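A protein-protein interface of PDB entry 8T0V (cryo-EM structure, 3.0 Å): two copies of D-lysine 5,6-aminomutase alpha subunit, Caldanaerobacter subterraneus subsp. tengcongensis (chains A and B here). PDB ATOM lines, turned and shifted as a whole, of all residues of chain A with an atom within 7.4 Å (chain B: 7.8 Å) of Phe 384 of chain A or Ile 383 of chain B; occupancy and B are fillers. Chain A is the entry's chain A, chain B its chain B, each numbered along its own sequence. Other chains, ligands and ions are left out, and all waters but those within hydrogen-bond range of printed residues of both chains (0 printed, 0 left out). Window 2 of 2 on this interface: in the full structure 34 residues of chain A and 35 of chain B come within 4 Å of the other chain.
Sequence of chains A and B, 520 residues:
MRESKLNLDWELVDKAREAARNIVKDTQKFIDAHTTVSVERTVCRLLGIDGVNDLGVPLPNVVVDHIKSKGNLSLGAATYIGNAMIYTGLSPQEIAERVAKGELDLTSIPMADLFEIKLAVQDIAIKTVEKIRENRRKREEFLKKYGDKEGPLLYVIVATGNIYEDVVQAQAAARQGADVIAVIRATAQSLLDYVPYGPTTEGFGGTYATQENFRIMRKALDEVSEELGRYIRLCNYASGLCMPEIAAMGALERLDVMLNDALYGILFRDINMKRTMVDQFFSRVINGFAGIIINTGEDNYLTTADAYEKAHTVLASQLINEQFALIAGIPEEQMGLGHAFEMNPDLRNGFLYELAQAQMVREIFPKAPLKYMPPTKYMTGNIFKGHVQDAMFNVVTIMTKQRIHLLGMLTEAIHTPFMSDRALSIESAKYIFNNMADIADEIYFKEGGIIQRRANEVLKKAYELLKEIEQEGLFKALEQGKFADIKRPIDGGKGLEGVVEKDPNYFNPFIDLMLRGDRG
Among the printed residues, merely in contact across the chains: Val 388 of chain A with His 387 of chain B, His 387 of chain A with Val 388 of chain B, His 387 of chain A with Phe 384 of chain B, Phe 384 of chain A with His 387 of chain B, Leu 410 of chain A with Phe 384 of chain B, Val 388 of chain A with Ser 428 of chain B and Phe 384 of chain A with Ile 383 of chain B.
The side-chain carboxylate (OD2) of Asp 390 of chain A lies within hydrogen-bond range of the backbone NH (N) of Leu 410 of chain A, 3.3 Å away.
Phe 384 of chain A touches Ile 383 of chain B, but with the chains exchanged Ile 383 of chain A does not touch Phe 384 of chain B (4.2 Å). Phe 384 of chain A touches His 387 of chain B, and with the chains exchanged His 387 of chain A touches Phe 384 of chain B. His 387 of chain A touches Val 388 of chain B, and with the chains exchanged Val 388 of chain A touches His 387 of chain B. Leu 410 of chain A touches Phe 384 of chain B, but with the chains exchanged Phe 384 of chain A does not touch Leu 410 of chain B (4.1 Å).
Hydrophobic or aromatic side chains of chain A that line the printed part of chain B: Phe 384, His 387, Val 388 and Leu 410. Of the 25 printed residues of chain B, 6 touch a printed residue of chain A. Printed residues of chain B that touch a printed residue of chain A: Ile 383, Phe 384, His 387, Val 388, Glu 427 and Ser 428. Hydrophobic or aromatic side chains of chain B within 4 Å of the printed part of chain A: Ile 383, Phe 384, His 387 and Val 388. Among the printed residues, no Asp or Glu carboxylate lies within 4 Å of a Lys or Arg side-chain nitrogen of the other chain.
The side-chain carboxylate (OE1) of Glu 427 of chain B lies within hydrogen-bond range of the side-chain amide nitrogen (ND2) of Asn 382 of chain A (2.8 Å).
Of the printed residues of chain B, Phe 384 of chain A touches Ile 383 (3.998 Å) and His 387 (3.6 Å). Of the printed residues of chain B, Leu 410 of chain A touches Phe 384 (3.96 Å). Leu 424 of chain A touches none of the printed residues of chain B. Of the printed residues of chain A, Ile 383 of chain B touches Phe 384. Of the printed residues of chain A, Val 388 of chain B touches His 387. Ser 420 of chain B touches none of the printed residues of chain A. The nearest printed residue of chain B that does not touch Phe 384 of chain A is Phe 384 of chain B (4.01 Å). The nearest printed residue of chain A that does not touch Ile 383 of chain B is His 387 of chain A (6.4 Å). The nearest printed residue of chain A that does not touch Phe 384 of chain B is Phe 384 of chain A (4.01 Å).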
ATOM      1  N   THR A 380      18.000  -6.979  34.375  1.00  0.00           N
ATOM      2  CA  THR A 380      17.345  -7.142  35.667  1.00  0.00           C
ATOM      3  C   THR A 380      17.564  -8.576  36.143  1.00  0.00           C
ATOM      4  O   THR A 380      18.384  -9.317  35.594  1.00  0.00           O
ATOM      5  CB  THR A 380      15.855  -6.791  35.565  1.00  0.00           C
ATOM      6  OG1 THR A 380      15.273  -7.482  34.454  1.00  0.00           O
ATOM      7  CG2 THR A 380      15.676  -5.298  35.374  1.00  0.00           C
ATOM      8  N   GLY A 381      16.829  -8.961  37.187  1.00  0.00           N
ATOM      9  CA  GLY A 381      16.904 -10.306  37.721  1.00  0.00           C
ATOM     10  C   GLY A 381      16.083 -11.334  36.979  1.00  0.00           C
ATOM     11  O   GLY A 381      16.144 -12.516  37.322  1.00  0.00           O
ATOM     12  N   ASN A 382      15.311 -10.914  35.978  1.00  0.00           N
ATOM     13  CA  ASN A 382      14.554 -11.835  35.133  1.00  0.00           C
ATOM     14  C   ASN A 382      15.516 -12.415  34.103  1.00  0.00           C
ATOM     15  O   ASN A 382      15.759 -11.851  33.036  1.00  0.00           O
ATOM     16  CB  ASN A 382      13.382 -11.117  34.476  1.00  0.00           C
ATOM     17  CG  ASN A 382      12.332 -12.070  33.955  1.00  0.00           C
ATOM     18  OD1 ASN A 382      12.373 -13.268  34.227  1.00  0.00           O
ATOM     19  ND2 ASN A 382      11.380 -11.542  33.204  1.00  0.00           N
ATOM     20  N   ILE A 383      16.089 -13.568  34.447  1.00  0.00           N
ATOM     21  CA  ILE A 383      17.112 -14.158  33.591  1.00  0.00           C
ATOM     22  C   ILE A 383      16.529 -14.582  32.249  1.00  0.00           C
ATOM     23  O   ILE A 383      17.249 -14.654  31.246  1.00  0.00           O
ATOM     24  CB  ILE A 383      17.797 -15.331  34.321  1.00  0.00           C
ATOM     25  CG1 ILE A 383      16.804 -16.452  34.613  1.00  0.00           C
ATOM     26  CG2 ILE A 383      18.427 -14.845  35.608  1.00  0.00           C
ATOM     27  CD1 ILE A 383      17.409 -17.620  35.333  1.00  0.00           C
ATOM     28  N   PHE A 384      15.227 -14.862  32.196  1.00  0.00           N
ATOM     29  CA  PHE A 384      14.617 -15.300  30.944  1.00  0.00           C
ATOM     30  C   PHE A 384      14.522 -14.154  29.941  1.00  0.00           C
ATOM     31  O   PHE A 384      14.897 -14.301  28.768  1.00  0.00           O
ATOM     32  CB  PHE A 384      13.244 -15.902  31.234  1.00  0.00           C
ATOM     33  CG  PHE A 384      13.285 -17.046  32.204  1.00  0.00           C
ATOM     34  CD1 PHE A 384      13.602 -18.323  31.776  1.00  0.00           C
ATOM     35  CD2 PHE A 384      13.031 -16.841  33.546  1.00  0.00           C
ATOM     36  CE1 PHE A 384      13.651 -19.370  32.663  1.00  0.00           C
ATOM     37  CE2 PHE A 384      13.080 -17.889  34.438  1.00  0.00           C
ATOM     38  CZ  PHE A 384      13.391 -19.152  33.995  1.00  0.00           C
ATOM     39  N   LYS A 385      14.036 -12.994  30.382  1.00  0.00           N
ATOM     40  CA  LYS A 385      14.034 -11.845  29.489  1.00  0.00           C
ATOM     41  C   LYS A 385      15.452 -11.393  29.179  1.00  0.00           C
ATOM     42  O   LYS A 385      15.704 -10.839  28.106  1.00  0.00           O
ATOM     43  CB  LYS A 385      13.230 -10.694  30.083  1.00  0.00           C
ATOM     44  CG  LYS A 385      12.697  -9.757  29.015  1.00  0.00           C
ATOM     45  CD  LYS A 385      12.175  -8.459  29.584  1.00  0.00           C
ATOM     46  CE  LYS A 385      11.972  -7.438  28.480  1.00  0.00           C
ATOM     47  NZ  LYS A 385      11.704  -6.078  29.006  1.00  0.00           N
ATOM     48  N   GLY A 386      16.394 -11.622  30.097  1.00  0.00           N
ATOM     49  CA  GLY A 386      17.789 -11.358  29.782  1.00  0.00           C
ATOM     50  C   GLY A 386      18.289 -12.217  28.640  1.00  0.00           C
ATOM     51  O   GLY A 386      18.986 -11.735  27.744  1.00  0.00           O
ATOM     52  N   HIS A 387      17.935 -13.501  28.652  1.00  0.00           N
ATOM     53  CA  HIS A 387      18.291 -14.386  27.549  1.00  0.00           C
ATOM     54  C   HIS A 387      17.669 -13.900  26.247  1.00  0.00           C
ATOM     55  O   HIS A 387      18.302 -13.939  25.186  1.00  0.00           O
ATOM     56  CB  HIS A 387      17.837 -15.811  27.865  1.00  0.00           C
ATOM     57  CG  HIS A 387      18.799 -16.871  27.430  1.00  0.00           C
ATOM     58  ND1 HIS A 387      20.144 -16.822  27.724  1.00  0.00           N
ATOM     59  CD2 HIS A 387      18.608 -18.020  26.742  1.00  0.00           C
ATOM     60  CE1 HIS A 387      20.740 -17.889  27.225  1.00  0.00           C
ATOM     61  NE2 HIS A 387      19.830 -18.632  26.624  1.00  0.00           N
ATOM     62  N   VAL A 388      16.419 -13.442  26.309  1.00  0.00           N
ATOM     63  CA  VAL A 388      15.755 -12.947  25.100  1.00  0.00           C
ATOM     64  C   VAL A 388      16.454 -11.696  24.565  1.00  0.00           C
ATOM     65  O   VAL A 388      16.645 -11.540  23.350  1.00  0.00           O
ATOM     66  CB  VAL A 388      14.264 -12.693  25.390  1.00  0.00           C
ATOM     67  CG1 VAL A 388      13.607 -11.965  24.231  1.00  0.00           C
ATOM     68  CG2 VAL A 388      13.559 -14.008  25.671  1.00  0.00           C
ATOM     69  N   GLN A 389      16.830 -10.779  25.457  1.00  0.00           N
ATOM     70  CA  GLN A 389      17.537  -9.572  25.036  1.00  0.00           C
ATOM     71  C   GLN A 389      18.882  -9.917  24.407  1.00  0.00           C
ATOM     72  O   GLN A 389      19.284  -9.321  23.401  1.00  0.00           O
ATOM     73  CB  GLN A 389      17.733  -8.643  26.232  1.00  0.00           C
ATOM     74  CG  GLN A 389      16.453  -8.086  26.811  1.00  0.00           C
ATOM     75  CD  GLN A 389      16.708  -7.129  27.949  1.00  0.00           C
ATOM     76  OE1 GLN A 389      17.569  -6.260  27.857  1.00  0.00           O
ATOM     77  NE2 GLN A 389      15.961  -7.281  29.028  1.00  0.00           N
ATOM     78  N   ASP A 390      19.598 -10.875  24.998  1.00  0.00           N
ATOM     79  CA  ASP A 390      20.852 -11.327  24.406  1.00  0.00           C
ATOM     80  C   ASP A 390      20.623 -11.927  23.030  1.00  0.00           C
ATOM     81  O   ASP A 390      21.444 -11.754  22.123  1.00  0.00           O
ATOM     82  CB  ASP A 390      21.523 -12.350  25.315  1.00  0.00           C
ATOM     83  CG  ASP A 390      21.779 -11.816  26.696  1.00  0.00           C
ATOM     84  OD1 ASP A 390      21.755 -10.584  26.873  1.00  0.00           O
ATOM     85  OD2 ASP A 390      22.009 -12.634  27.607  1.00  0.00           O
ATOM     86  N   LEU A 410      22.654 -13.916  30.617  1.00  0.00           N
ATOM     87  CA  LEU A 410      21.319 -13.709  31.165  1.00  0.00           C
ATOM     88  C   LEU A 410      21.374 -13.208  32.601  1.00  0.00           C
ATOM     89  O   LEU A 410      20.436 -12.549  33.065  1.00  0.00           O
ATOM     90  CB  LEU A 410      20.514 -15.008  31.074  1.00  0.00           C
ATOM     91  CG  LEU A 410      20.870 -16.186  31.990  1.00  0.00           C
ATOM     92  CD1 LEU A 410      19.870 -17.308  31.805  1.00  0.00           C
ATOM     93  CD2 LEU A 410      22.271 -16.701  31.738  1.00  0.00           C
ATOM     94  N   LEU A 424      25.204 -21.474  28.298  1.00  0.00           N
ATOM     95  CA  LEU A 424      23.931 -21.100  27.692  1.00  0.00           C
ATOM     96  C   LEU A 424      24.110 -19.960  26.698  1.00  0.00           C
ATOM     97  O   LEU A 424      23.534 -19.976  25.604  1.00  0.00           O
ATOM     98  CB  LEU A 424      22.929 -20.719  28.782  1.00  0.00           C
ATOM     99  CG  LEU A 424      22.583 -21.850  29.751  1.00  0.00           C
ATOM    100  CD1 LEU A 424      21.970 -21.307  31.027  1.00  0.00           C
ATOM    101  CD2 LEU A 424      21.658 -22.850  29.089  1.00  0.00           C
ATOM    102  N   MET B 379      11.457 -29.185  20.149  1.00  0.00           N
ATOM    103  CA  MET B 379      11.600 -28.595  21.472  1.00  0.00           C
ATOM    104  C   MET B 379      12.132 -29.639  22.446  1.00  0.00           C
ATOM    105  O   MET B 379      11.615 -30.757  22.512  1.00  0.00           O
ATOM    106  CB  MET B 379      10.245 -28.082  21.946  1.00  0.00           C
ATOM    107  CG  MET B 379      10.277 -26.756  22.659  1.00  0.00           C
ATOM    108  SD  MET B 379      10.241 -25.372  21.516  1.00  0.00           S
ATOM    109  CE  MET B 379      10.633 -24.050  22.638  1.00  0.00           C
ATOM    110  N   THR B 380      13.154 -29.280  23.211  1.00  0.00           N
ATOM    111  CA  THR B 380      13.798 -30.203  24.138  1.00  0.00           C
ATOM    112  C   THR B 380      13.629 -29.705  25.575  1.00  0.00           C
ATOM    113  O   THR B 380      12.876 -28.766  25.848  1.00  0.00           O
ATOM    114  CB  THR B 380      15.276 -30.393  23.782  1.00  0.00           C
ATOM    115  OG1 THR B 380      16.052 -29.329  24.344  1.00  0.00           O
ATOM    116  CG2 THR B 380      15.473 -30.428  22.275  1.00  0.00           C
ATOM    117  N   GLY B 381      14.330 -30.358  26.499  1.00  0.00           N
ATOM    118  CA  GLY B 381      14.222 -30.028  27.907  1.00  0.00           C
ATOM    119  C   GLY B 381      14.997 -28.800  28.327  1.00  0.00           C
ATOM    120  O   GLY B 381      14.956 -28.440  29.508  1.00  0.00           O
ATOM    121  N   ASN B 382      15.716 -28.167  27.403  1.00  0.00           N
ATOM    122  CA  ASN B 382      16.391 -26.910  27.694  1.00  0.00           C
ATOM    123  C   ASN B 382      15.387 -25.770  27.616  1.00  0.00           C
ATOM    124  O   ASN B 382      15.007 -25.340  26.525  1.00  0.00           O
ATOM    125  CB  ASN B 382      17.547 -26.682  26.721  1.00  0.00           C
ATOM    126  CG  ASN B 382      18.655 -25.847  27.318  1.00  0.00           C
ATOM    127  OD1 ASN B 382      18.559 -25.387  28.453  1.00  0.00           O
ATOM    128  ND2 ASN B 382      19.720 -25.656  26.562  1.00  0.00           N
ATOM    129  N   ILE B 383      14.940 -25.285  28.773  1.00  0.00           N
ATOM    130  CA  ILE B 383      13.934 -24.231  28.790  1.00  0.00           C
ATOM    131  C   ILE B 383      14.516 -22.926  28.257  1.00  0.00           C
ATOM    132  O   ILE B 383      13.794 -22.086  27.708  1.00  0.00           O
ATOM    133  CB  ILE B 383      13.354 -24.075  30.209  1.00  0.00           C
ATOM    134  CG1 ILE B 383      14.425 -23.662  31.214  1.00  0.00           C
ATOM    135  CG2 ILE B 383      12.712 -25.374  30.655  1.00  0.00           C
ATOM    136  CD1 ILE B 383      13.870 -23.361  32.585  1.00  0.00           C
ATOM    137  N   PHE B 384      15.830 -22.746  28.385  1.00  0.00           N
ATOM    138  CA  PHE B 384      16.457 -21.493  27.972  1.00  0.00           C
ATOM    139  C   PHE B 384      16.607 -21.417  26.454  1.00  0.00           C
ATOM    140  O   PHE B 384      16.229 -20.416  25.826  1.00  0.00           O
ATOM    141  CB  PHE B 384      17.805 -21.348  28.676  1.00  0.00           C
ATOM    142  CG  PHE B 384      17.723 -21.511  30.166  1.00  0.00           C
ATOM    143  CD1 PHE B 384      17.800 -22.764  30.746  1.00  0.00           C
ATOM    144  CD2 PHE B 384      17.555 -20.413  30.989  1.00  0.00           C
ATOM    145  CE1 PHE B 384      17.711 -22.917  32.114  1.00  0.00           C
ATOM    146  CE2 PHE B 384      17.469 -20.562  32.360  1.00  0.00           C
ATOM    147  CZ  PHE B 384      17.549 -21.817  32.920  1.00  0.00           C
ATOM    148  N   LYS B 385      17.139 -22.470  25.833  1.00  0.00           N
ATOM    149  CA  LYS B 385      17.144 -22.489  24.377  1.00  0.00           C
ATOM    150  C   LYS B 385      15.726 -22.518  23.829  1.00  0.00           C
ATOM    151  O   LYS B 385      15.482 -22.039  22.720  1.00  0.00           O
ATOM    152  CB  LYS B 385      17.938 -23.677  23.840  1.00  0.00           C
ATOM    153  CG  LYS B 385      18.266 -23.517  22.361  1.00  0.00           C
ATOM    154  CD  LYS B 385      18.891 -24.747  21.741  1.00  0.00           C
ATOM    155  CE  LYS B 385      18.968 -24.584  20.230  1.00  0.00           C
ATOM    156  NZ  LYS B 385      19.502 -25.777  19.528  1.00  0.00           N
ATOM    157  N   GLY B 386      14.778 -23.066  24.588  1.00  0.00           N
ATOM    158  CA  GLY B 386      13.391 -23.012  24.160  1.00  0.00           C
ATOM    159  C   GLY B 386      12.850 -21.597  24.138  1.00  0.00           C
ATOM    160  O   GLY B 386      12.135 -21.207  23.214  1.00  0.00           O
ATOM    161  N   HIS B 387      13.186 -20.808  25.158  1.00  0.00           N
ATOM    162  CA  HIS B 387      12.834 -19.392  25.156  1.00  0.00           C
ATOM    163  C   HIS B 387      13.441 -18.690  23.947  1.00  0.00           C
ATOM    164  O   HIS B 387      12.798 -17.847  23.310  1.00  0.00           O
ATOM    165  CB  HIS B 387      13.314 -18.743  26.459  1.00  0.00           C
ATOM    166  CG  HIS B 387      12.305 -17.843  27.103  1.00  0.00           C
ATOM    167  ND1 HIS B 387      11.022 -18.249  27.396  1.00  0.00           N
ATOM    168  CD2 HIS B 387      12.398 -16.561  27.525  1.00  0.00           C
ATOM    169  CE1 HIS B 387      10.365 -17.254  27.963  1.00  0.00           C
ATOM    170  NE2 HIS B 387      11.176 -16.217  28.052  1.00  0.00           N
ATOM    171  N   VAL B 388      14.683 -19.034  23.608  1.00  0.00           N
ATOM    172  CA  VAL B 388      15.336 -18.422  22.447  1.00  0.00           C
ATOM    173  C   VAL B 388      14.612 -18.799  21.154  1.00  0.00           C
ATOM    174  O   VAL B 388      14.401 -17.960  20.266  1.00  0.00           O
ATOM    175  CB  VAL B 388      16.821 -18.821  22.402  1.00  0.00           C
ATOM    176  CG1 VAL B 388      17.439 -18.425  21.082  1.00  0.00           C
ATOM    177  CG2 VAL B 388      17.566 -18.176  23.548  1.00  0.00           C
ATOM    178  N   GLN B 389      14.241 -20.073  21.016  1.00  0.00           N
ATOM    179  CA  GLN B 389      13.533 -20.518  19.819  1.00  0.00           C
ATOM    180  C   GLN B 389      12.186 -19.820  19.691  1.00  0.00           C
ATOM    181  O   GLN B 389      11.766 -19.439  18.591  1.00  0.00           O
ATOM    182  CB  GLN B 389      13.346 -22.034  19.851  1.00  0.00           C
ATOM    183  CG  GLN B 389      14.629 -22.836  19.734  1.00  0.00           C
ATOM    184  CD  GLN B 389      14.370 -24.322  19.613  1.00  0.00           C
ATOM    185  OE1 GLN B 389      13.621 -24.760  18.744  1.00  0.00           O
ATOM    186  NE2 GLN B 389      14.987 -25.105  20.484  1.00  0.00           N
ATOM    187  N   ASP B 390      11.485 -19.649  20.813  1.00  0.00           N
ATOM    188  CA  ASP B 390      10.233 -18.900  20.798  1.00  0.00           C
ATOM    189  C   ASP B 390      10.460 -17.450  20.398  1.00  0.00           C
ATOM    190  O   ASP B 390       9.621 -16.846  19.722  1.00  0.00           O
ATOM    191  CB  ASP B 390       9.568 -18.967  22.166  1.00  0.00           C
ATOM    192  CG  ASP B 390       9.283 -20.376  22.600  1.00  0.00           C
ATOM    193  OD1 ASP B 390       9.065 -21.236  21.726  1.00  0.00           O
ATOM    194  OD2 ASP B 390       9.273 -20.623  23.820  1.00  0.00           O
ATOM    195  N   MET B 409       5.558 -21.957  24.367  1.00  0.00           N
ATOM    196  CA  MET B 409       5.816 -21.994  25.798  1.00  0.00           C
ATOM    197  C   MET B 409       7.237 -22.452  26.085  1.00  0.00           C
ATOM    198  O   MET B 409       7.787 -23.313  25.395  1.00  0.00           O
ATOM    199  CB  MET B 409       4.820 -22.901  26.518  1.00  0.00           C
ATOM    200  CG  MET B 409       3.382 -22.486  26.302  1.00  0.00           C
ATOM    201  SD  MET B 409       2.787 -21.310  27.525  1.00  0.00           S
ATOM    202  CE  MET B 409       2.282 -19.963  26.462  1.00  0.00           C
ATOM    203  N   LEU B 410       7.817 -21.834  27.109  1.00  0.00           N
ATOM    204  CA  LEU B 410       9.131 -22.199  27.617  1.00  0.00           C
ATOM    205  C   LEU B 410       9.300 -23.710  27.739  1.00  0.00           C
ATOM    206  O   LEU B 410      10.342 -24.262  27.374  1.00  0.00           O
ATOM    207  CB  LEU B 410       9.301 -21.516  28.976  1.00  0.00           C
ATOM    208  CG  LEU B 410      10.580 -21.688  29.767  1.00  0.00           C
ATOM    209  CD1 LEU B 410      11.690 -20.879  29.146  1.00  0.00           C
ATOM    210  CD2 LEU B 410      10.345 -21.271  31.198  1.00  0.00           C
ATOM    211  N   THR B 411       8.265 -24.394  28.230  1.00  0.00           N
ATOM    212  CA  THR B 411       8.342 -25.792  28.642  1.00  0.00           C
ATOM    213  C   THR B 411       7.401 -26.680  27.835  1.00  0.00           C
ATOM    214  O   THR B 411       6.665 -27.486  28.401  1.00  0.00           O
ATOM    215  CB  THR B 411       8.023 -25.921  30.128  1.00  0.00           C
ATOM    216  OG1 THR B 411       6.705 -25.420  30.371  1.00  0.00           O
ATOM    217  CG2 THR B 411       9.014 -25.131  30.955  1.00  0.00           C
ATOM    218  N   GLU B 412       7.404 -26.537  26.507  1.00  0.00           N
ATOM    219  CA  GLU B 412       6.522 -27.352  25.681  1.00  0.00           C
ATOM    220  C   GLU B 412       6.836 -28.833  25.814  1.00  0.00           C
ATOM    221  O   GLU B 412       5.920 -29.652  25.943  1.00  0.00           O
ATOM    222  CB  GLU B 412       6.630 -26.931  24.218  1.00  0.00           C
ATOM    223  CG  GLU B 412       5.902 -25.639  23.881  1.00  0.00           C
ATOM    224  CD  GLU B 412       5.832 -25.378  22.387  1.00  0.00           C
ATOM    225  OE1 GLU B 412       5.254 -26.215  21.664  1.00  0.00           O
ATOM    226  OE2 GLU B 412       6.361 -24.343  21.933  1.00  0.00           O
ATOM    227  N   ALA B 413       8.116 -29.201  25.791  1.00  0.00           N
ATOM    228  CA  ALA B 413       8.491 -30.608  25.801  1.00  0.00           C
ATOM    229  C   ALA B 413       8.262 -31.280  27.146  1.00  0.00           C
ATOM    230  O   ALA B 413       8.357 -32.508  27.223  1.00  0.00           O
ATOM    231  CB  ALA B 413       9.958 -30.760  25.406  1.00  0.00           C
ATOM    232  N   ILE B 414       7.962 -30.521  28.196  1.00  0.00           N
ATOM    233  CA  ILE B 414       7.878 -31.047  29.556  1.00  0.00           C
ATOM    234  C   ILE B 414       6.428 -31.278  29.969  1.00  0.00           C
ATOM    235  O   ILE B 414       6.025 -32.408  30.246  1.00  0.00           O
ATOM    236  CB  ILE B 414       8.598 -30.117  30.557  1.00  0.00           C
ATOM    237  CG1 ILE B 414       9.926 -29.631  29.976  1.00  0.00           C
ATOM    238  CG2 ILE B 414       8.831 -30.840  31.867  1.00  0.00           C
ATOM    239  CD1 ILE B 414      10.651 -28.656  30.859  1.00  0.00           C
ATOM    240  N   HIS B 415       5.628 -30.218  30.012  1.00  0.00           N
ATOM    241  CA  HIS B 415       4.279 -30.311  30.547  1.00  0.00           C
ATOM    242  C   HIS B 415       3.444 -29.172  29.989  1.00  0.00           C
ATOM    243  O   HIS B 415       3.947 -28.285  29.297  1.00  0.00           O
ATOM    244  CB  HIS B 415       4.288 -30.279  32.078  1.00  0.00           C
ATOM    245  CG  HIS B 415       5.084 -29.151  32.663  1.00  0.00           C
ATOM    246  ND1 HIS B 415       4.857 -27.829  32.346  1.00  0.00           N
ATOM    247  CD2 HIS B 415       6.098 -29.150  33.560  1.00  0.00           C
ATOM    248  CE1 HIS B 415       5.704 -27.066  33.010  1.00  0.00           C
ATOM    249  NE2 HIS B 415       6.468 -27.844  33.755  1.00  0.00           N
ATOM    250  N   SER B 420       3.304 -19.265  35.326  1.00  0.00           N
ATOM    251  CA  SER B 420       4.526 -18.499  35.111  1.00  0.00           C
ATOM    252  C   SER B 420       5.070 -18.689  33.702  1.00  0.00           C
ATOM    253  O   SER B 420       5.611 -17.749  33.115  1.00  0.00           O
ATOM    254  CB  SER B 420       5.571 -18.891  36.151  1.00  0.00           C
ATOM    255  OG  SER B 420       5.581 -20.289  36.368  1.00  0.00           O
ATOM    256  N   ASP B 421       4.946 -19.891  33.140  1.00  0.00           N
ATOM    257  CA  ASP B 421       5.394 -20.100  31.768  1.00  0.00           C
ATOM    258  C   ASP B 421       4.598 -19.234  30.802  1.00  0.00           C
ATOM    259  O   ASP B 421       5.160 -18.630  29.881  1.00  0.00           O
ATOM    260  CB  ASP B 421       5.274 -21.574  31.386  1.00  0.00           C
ATOM    261  CG  ASP B 421       5.854 -22.503  32.431  1.00  0.00           C
ATOM    262  OD1 ASP B 421       6.585 -22.029  33.324  1.00  0.00           O
ATOM    263  OD2 ASP B 421       5.581 -23.718  32.355  1.00  0.00           O
ATOM    264  N   LEU B 424       5.728 -15.594  31.174  1.00  0.00           N
ATOM    265  CA  LEU B 424       7.010 -15.358  30.518  1.00  0.00           C
ATOM    266  C   LEU B 424       6.854 -15.318  29.002  1.00  0.00           C
ATOM    267  O   LEU B 424       7.467 -14.485  28.325  1.00  0.00           O
ATOM    268  CB  LEU B 424       8.011 -16.437  30.927  1.00  0.00           C
ATOM    269  CG  LEU B 424       8.368 -16.530  32.411  1.00  0.00           C
ATOM    270  CD1 LEU B 424       9.105 -17.819  32.686  1.00  0.00           C
ATOM    271  CD2 LEU B 424       9.195 -15.349  32.862  1.00  0.00           C
ATOM    272  N   SER B 425       6.044 -16.219  28.448  1.00  0.00           N
ATOM    273  CA  SER B 425       5.833 -16.225  27.004  1.00  0.00           C
ATOM    274  C   SER B 425       5.184 -14.928  26.541  1.00  0.00           C
ATOM    275  O   SER B 425       5.613 -14.321  25.552  1.00  0.00           O
ATOM    276  CB  SER B 425       4.973 -17.424  26.613  1.00  0.00           C
ATOM    277  OG  SER B 425       5.501 -18.615  27.163  1.00  0.00           O
ATOM    278  N   GLU B 427       5.260 -12.048  28.026  1.00  0.00           N
ATOM    279  CA  GLU B 427       6.202 -10.952  28.221  1.00  0.00           C
ATOM    280  C   GLU B 427       7.217 -10.883  27.086  1.00  0.00           C
ATOM    281  O   GLU B 427       7.484  -9.806  26.538  1.00  0.00           O
ATOM    282  CB  GLU B 427       6.897 -11.137  29.567  1.00  0.00           C
ATOM    283  CG  GLU B 427       8.130 -10.305  29.788  1.00  0.00           C
ATOM    284  CD  GLU B 427       8.661 -10.460  31.197  1.00  0.00           C
ATOM    285  OE1 GLU B 427       9.059 -11.589  31.553  1.00  0.00           O
ATOM    286  OE2 GLU B 427       8.674  -9.462  31.946  1.00  0.00           O
ATOM    287  N   SER B 428       7.793 -12.027  26.718  1.00  0.00           N
ATOM    288  CA  SER B 428       8.754 -12.052  25.620  1.00  0.00           C
ATOM    289  C   SER B 428       8.111 -11.619  24.310  1.00  0.00           C
ATOM    290  O   SER B 428       8.695 -10.836  23.548  1.00  0.00           O
ATOM    291  CB  SER B 428       9.345 -13.454  25.489  1.00  0.00           C
ATOM    292  OG  SER B 428       9.895 -13.663  24.205  1.00  0.00           O
